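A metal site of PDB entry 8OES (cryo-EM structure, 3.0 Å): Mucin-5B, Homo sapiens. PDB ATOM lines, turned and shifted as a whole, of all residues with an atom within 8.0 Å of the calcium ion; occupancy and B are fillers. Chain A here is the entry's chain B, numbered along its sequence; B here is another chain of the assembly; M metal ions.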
ATOM      1  N   THR A 880     -12.922  18.645  25.341  1.00  0.00           N
ATOM      2  CA  THR A 880     -14.282  18.162  25.421  1.00  0.00           C
ATOM      3  C   THR A 880     -14.343  16.813  26.133  1.00  0.00           C
ATOM      4  O   THR A 880     -13.342  16.298  26.627  1.00  0.00           O
ATOM      5  CB  THR A 880     -14.893  18.040  24.034  1.00  0.00           C
ATOM      6  OG1 THR A 880     -15.941  17.068  24.076  1.00  0.00           O
ATOM      7  CG2 THR A 880     -13.871  17.595  23.046  1.00  0.00           C
ATOM      8  N   PHE A 881     -15.556  16.271  26.194  1.00  0.00           N
ATOM      9  CA  PHE A 881     -15.783  15.036  26.931  1.00  0.00           C
ATOM     10  C   PHE A 881     -15.017  13.873  26.306  1.00  0.00           C
ATOM     11  O   PHE A 881     -14.462  13.042  27.021  1.00  0.00           O
ATOM     12  CB  PHE A 881     -17.276  14.723  26.950  1.00  0.00           C
ATOM     13  CG  PHE A 881     -18.054  15.488  27.994  1.00  0.00           C
ATOM     14  CD1 PHE A 881     -17.870  15.238  29.330  1.00  0.00           C
ATOM     15  CD2 PHE A 881     -18.995  16.424  27.610  1.00  0.00           C
ATOM     16  CE1 PHE A 881     -18.601  15.925  30.273  1.00  0.00           C
ATOM     17  CE2 PHE A 881     -19.717  17.113  28.556  1.00  0.00           C
ATOM     18  CZ  PHE A 881     -19.525  16.857  29.875  1.00  0.00           C
ATOM     19  N   ASP A 882     -15.002  13.807  24.971  1.00  0.00           N
ATOM     20  CA  ASP A 882     -14.358  12.722  24.242  1.00  0.00           C
ATOM     21  C   ASP A 882     -12.845  12.875  24.149  1.00  0.00           C
ATOM     22  O   ASP A 882     -12.225  12.153  23.376  1.00  0.00           O
ATOM     23  CB  ASP A 882     -14.926  12.630  22.830  1.00  0.00           C
ATOM     24  CG  ASP A 882     -16.398  12.312  22.826  1.00  0.00           C
ATOM     25  OD1 ASP A 882     -16.820  11.389  23.552  1.00  0.00           O
ATOM     26  OD2 ASP A 882     -17.139  12.982  22.095  1.00  0.00           O
ATOM     27  N   ASP A 884     -11.017  15.368  22.955  1.00  0.00           N
ATOM     28  CA  ASP A 884     -10.480  16.277  21.963  1.00  0.00           C
ATOM     29  C   ASP A 884     -10.083  17.601  22.613  1.00  0.00           C
ATOM     30  O   ASP A 884     -10.660  18.019  23.612  1.00  0.00           O
ATOM     31  CB  ASP A 884     -11.494  16.516  20.847  1.00  0.00           C
ATOM     32  CG  ASP A 884     -10.903  17.262  19.683  1.00  0.00           C
ATOM     33  OD1 ASP A 884      -9.691  17.526  19.694  1.00  0.00           O
ATOM     34  OD2 ASP A 884     -11.662  17.588  18.742  1.00  0.00           O
ATOM     35  N   GLY A 995     -23.648  10.450  24.748  1.00  0.00           N
ATOM     36  CA  GLY A 995     -24.185  10.534  23.403  1.00  0.00           C
ATOM     37  C   GLY A 995     -25.371  11.463  23.235  1.00  0.00           C
ATOM     38  O   GLY A 995     -25.788  11.686  22.091  1.00  0.00           O
ATOM     39  N   CYS A1001     -18.657  21.106  24.568  1.00  0.00           N
ATOM     40  CA  CYS A1001     -18.026  19.934  25.148  1.00  0.00           C
ATOM     41  C   CYS A1001     -18.311  18.679  24.329  1.00  0.00           C
ATOM     42  O   CYS A1001     -18.346  17.569  24.867  1.00  0.00           O
ATOM     43  CB  CYS A1001     -18.474  19.727  26.591  1.00  0.00           C
ATOM     44  SG  CYS A1001     -18.054  21.068  27.715  1.00  0.00           S
ATOM     45  N   GLY A1002     -18.521  18.838  23.024  1.00  0.00           N
ATOM     46  CA  GLY A1002     -18.758  17.710  22.171  1.00  0.00           C
ATOM     47  C   GLY A1002     -20.093  17.077  22.485  1.00  0.00           C
ATOM     48  O   GLY A1002     -20.932  17.631  23.184  1.00  0.00           O
ATOM     49  N   ASN A1003     -20.282  15.874  21.955  1.00  0.00           N
ATOM     50  CA  ASN A1003     -21.510  15.135  22.181  1.00  0.00           C
ATOM     51  C   ASN A1003     -21.294  13.900  23.046  1.00  0.00           C
ATOM     52  O   ASN A1003     -22.211  13.086  23.171  1.00  0.00           O
ATOM     53  CB  ASN A1003     -22.152  14.745  20.850  1.00  0.00           C
ATOM     54  CG  ASN A1003     -21.380  13.680  20.114  1.00  0.00           C
ATOM     55  OD1 ASN A1003     -20.156  13.623  20.194  1.00  0.00           O
ATOM     56  ND2 ASN A1003     -22.091  12.830  19.391  1.00  0.00           N
ATOM     57  N   PHE A1004     -20.122  13.762  23.658  1.00  0.00           N
ATOM     58  CA  PHE A1004     -19.871  12.694  24.618  1.00  0.00           C
ATOM     59  C   PHE A1004     -20.237  11.339  24.039  1.00  0.00           C
ATOM     60  O   PHE A1004     -21.135  10.646  24.521  1.00  0.00           O
ATOM     61  CB  PHE A1004     -20.629  12.962  25.910  1.00  0.00           C
ATOM     62  CG  PHE A1004     -20.195  12.111  27.071  1.00  0.00           C
ATOM     63  CD1 PHE A1004     -19.045  11.366  27.011  1.00  0.00           C
ATOM     64  CD2 PHE A1004     -20.936  12.084  28.231  1.00  0.00           C
ATOM     65  CE1 PHE A1004     -18.651  10.600  28.080  1.00  0.00           C
ATOM     66  CE2 PHE A1004     -20.546  11.321  29.308  1.00  0.00           C
ATOM     67  CZ  PHE A1004     -19.404  10.579  29.232  1.00  0.00           C
ATOM     68  N   ASP A1005     -19.548  10.962  22.960  1.00  0.00           N
ATOM     69  CA  ASP A1005     -19.844   9.707  22.275  1.00  0.00           C
ATOM     70  C   ASP A1005     -18.641   8.792  22.182  1.00  0.00           C
ATOM     71  O   ASP A1005     -18.712   7.763  21.495  1.00  0.00           O
ATOM     72  CB  ASP A1005     -20.392   9.994  20.867  1.00  0.00           C
ATOM     73  CG  ASP A1005     -19.423  10.785  20.015  1.00  0.00           C
ATOM     74  OD1 ASP A1005     -18.446  11.331  20.559  1.00  0.00           O
ATOM     75  OD2 ASP A1005     -19.631  10.856  18.787  1.00  0.00           O
ATOM     76  N   ASP A1006     -17.539   9.119  22.856  1.00  0.00           N
ATOM     77  CA  ASP A1006     -16.270   8.394  22.716  1.00  0.00           C
ATOM     78  C   ASP A1006     -15.848   8.324  21.253  1.00  0.00           C
ATOM     79  O   ASP A1006     -15.382   7.300  20.768  1.00  0.00           O
ATOM     80  CB  ASP A1006     -16.369   6.995  23.325  1.00  0.00           C
ATOM     81  CG  ASP A1006     -17.073   6.981  24.657  1.00  0.00           C
ATOM     82  OD1 ASP A1006     -18.236   7.434  24.708  1.00  0.00           O
ATOM     83  OD2 ASP A1006     -16.474   6.525  25.641  1.00  0.00           O
ATOM     84  N   ASN A1007     -16.023   9.437  20.552  1.00  0.00           N
ATOM     85  CA  ASN A1007     -15.617   9.557  19.154  1.00  0.00           C
ATOM     86  C   ASN A1007     -15.201  11.004  18.967  1.00  0.00           C
ATOM     87  O   ASN A1007     -16.031  11.869  18.681  1.00  0.00           O
ATOM     88  CB  ASN A1007     -16.743   9.160  18.219  1.00  0.00           C
ATOM     89  CG  ASN A1007     -16.364   9.292  16.759  1.00  0.00           C
ATOM     90  OD1 ASN A1007     -15.304   9.811  16.420  1.00  0.00           O
ATOM     91  ND2 ASN A1007     -17.242   8.820  15.879  1.00  0.00           N
ATOM     92  N   ALA A1008     -13.906  11.260  19.132  1.00  0.00           N
ATOM     93  CA  ALA A1008     -13.411  12.626  19.214  1.00  0.00           C
ATOM     94  C   ALA A1008     -13.217  13.272  17.851  1.00  0.00           C
ATOM     95  O   ALA A1008     -13.037  14.492  17.798  1.00  0.00           O
ATOM     96  CB  ALA A1008     -12.086  12.645  19.978  1.00  0.00           C
ATOM     97  N   ILE A1009     -13.241  12.505  16.774  1.00  0.00           N
ATOM     98  CA  ILE A1009     -13.004  13.102  15.459  1.00  0.00           C
ATOM     99  C   ILE A1009     -14.188  13.963  15.051  1.00  0.00           C
ATOM    100  O   ILE A1009     -14.018  15.026  14.451  1.00  0.00           O
ATOM    101  CB  ILE A1009     -12.704  12.003  14.422  1.00  0.00           C
ATOM    102  CG1 ILE A1009     -12.052  10.799  15.102  1.00  0.00           C
ATOM    103  CG2 ILE A1009     -11.783  12.557  13.344  1.00  0.00           C
ATOM    104  CD1 ILE A1009     -11.871   9.607  14.181  1.00  0.00           C
ATOM    105  N   ASN A1010     -15.411  13.510  15.353  1.00  0.00           N
ATOM    106  CA  ASN A1010     -16.620  14.193  14.926  1.00  0.00           C
ATOM    107  C   ASN A1010     -17.174  15.136  15.985  1.00  0.00           C
ATOM    108  O   ASN A1010     -18.285  15.650  15.820  1.00  0.00           O
ATOM    109  CB  ASN A1010     -17.686  13.170  14.542  1.00  0.00           C
ATOM    110  CG  ASN A1010     -18.601  12.808  15.683  1.00  0.00           C
ATOM    111  OD1 ASN A1010     -18.148  12.509  16.789  1.00  0.00           O
ATOM    112  ND2 ASN A1010     -19.905  12.869  15.440  1.00  0.00           N
ATOM    113  N   ASP A1011     -16.425  15.400  17.051  1.00  0.00           N
ATOM    114  CA  ASP A1011     -16.906  16.312  18.084  1.00  0.00           C
ATOM    115  C   ASP A1011     -17.013  17.740  17.603  1.00  0.00           C
ATOM    116  O   ASP A1011     -17.599  18.562  18.310  1.00  0.00           O
ATOM    117  CB  ASP A1011     -16.007  16.261  19.302  1.00  0.00           C
ATOM    118  CG  ASP A1011     -16.656  15.566  20.457  1.00  0.00           C
ATOM    119  OD1 ASP A1011     -17.649  14.858  20.215  1.00  0.00           O
ATOM    120  OD2 ASP A1011     -16.188  15.728  21.607  1.00  0.00           O
ATOM    121  N   PHE A1012     -16.469  18.074  16.445  1.00  0.00           N
ATOM    122  CA  PHE A1012     -16.697  19.377  15.850  1.00  0.00           C
ATOM    123  C   PHE A1012     -18.011  19.385  15.094  1.00  0.00           C
ATOM    124  O   PHE A1012     -18.054  19.749  13.917  1.00  0.00           O
ATOM    125  CB  PHE A1012     -15.559  19.757  14.917  1.00  0.00           C
ATOM    126  CG  PHE A1012     -14.374  20.351  15.616  1.00  0.00           C
ATOM    127  CD1 PHE A1012     -14.139  20.085  16.947  1.00  0.00           C
ATOM    128  CD2 PHE A1012     -13.507  21.175  14.937  1.00  0.00           C
ATOM    129  CE1 PHE A1012     -13.060  20.633  17.580  1.00  0.00           C
ATOM    130  CE2 PHE A1012     -12.430  21.731  15.567  1.00  0.00           C
ATOM    131  CZ  PHE A1012     -12.200  21.460  16.886  1.00  0.00           C
ATOM    132  N   ALA A1013     -19.093  18.985  15.749  1.00  0.00           N
ATOM    133  CA  ALA A1013     -20.414  18.917  15.153  1.00  0.00           C
ATOM    134  C   ALA A1013     -21.178  20.192  15.499  1.00  0.00           C
ATOM    135  O   ALA A1013     -21.481  20.435  16.669  1.00  0.00           O
ATOM    136  CB  ALA A1013     -21.172  17.686  15.630  1.00  0.00           C
ATOM    137  N   VAL A1019     -20.213  18.056  10.585  1.00  0.00           N
ATOM    138  CA  VAL A1019     -18.893  17.986  11.217  1.00  0.00           C
ATOM    139  C   VAL A1019     -17.876  18.722  10.371  1.00  0.00           C
ATOM    140  O   VAL A1019     -17.709  18.445   9.176  1.00  0.00           O
ATOM    141  CB  VAL A1019     -18.483  16.536  11.438  1.00  0.00           C
ATOM    142  CG1 VAL A1019     -16.991  16.448  11.671  1.00  0.00           C
ATOM    143  CG2 VAL A1019     -19.229  15.954  12.615  1.00  0.00           C
ATOM    144  N   GLN B 542     -12.581   4.467  16.035  1.00  0.00           N
ATOM    145  CA  GLN B 542     -13.177   5.805  16.148  1.00  0.00           C
ATOM    146  C   GLN B 542     -13.325   6.222  17.613  1.00  0.00           C
ATOM    147  O   GLN B 542     -14.416   6.493  18.114  1.00  0.00           O
ATOM    148  CB  GLN B 542     -14.517   5.847  15.403  1.00  0.00           C
ATOM    149  CG  GLN B 542     -14.484   5.192  14.048  1.00  0.00           C
ATOM    150  CD  GLN B 542     -13.270   5.582  13.237  1.00  0.00           C
ATOM    151  OE1 GLN B 542     -12.819   6.723  13.274  1.00  0.00           O
ATOM    152  NE2 GLN B 542     -12.748   4.638  12.475  1.00  0.00           N
HETATM  153 CA    CA M   1     -18.111  12.848  19.062  1.00  0.00          CA
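The calcium ion is bound by OD1 of Asp 1005, OD1 of Asn 1010, O of Asn 1007, OD1 of Asp 1011, OD1 of Asn 1003 and OD2 of Asp 1005.
OD2 of Asp 882 lies close to OD1 of Asp 1011, at 2.7 Å.
The backbone NH (N) of Ile 1009 lies close to the side-chain amide oxygen (OD1) of Asn 1007 (3.4 Å).
O of Asn 1003 lies close to N of Gly 995 (3.4 Å).
OD1 of Asp 882 is in hydrogen-bond range of N of Asp 1006 (2.5 Å).
The side-chain carboxylate (OD2) of Asp 882 sits at hydrogen-bond distance from the backbone NH (N) of Phe 1004.
OD1 of Asp 882 sits at hydrogen-bond distance from N of Asp 1005 (2.8 Å).
OG1 of Thr 880 lies within hydrogen-bond range of OD2 of Asp 1011.
Merely in contact with the calcium ion: Asp 882.
Within 4 Å of the calcium ion: Asp 882, Asn 1003, Asp 1005, Asn 1007, Asn 1010 and Asp 1011.
The nearest printed residue that does not touch the calcium ion is Ala 1008 (4.5 Å).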
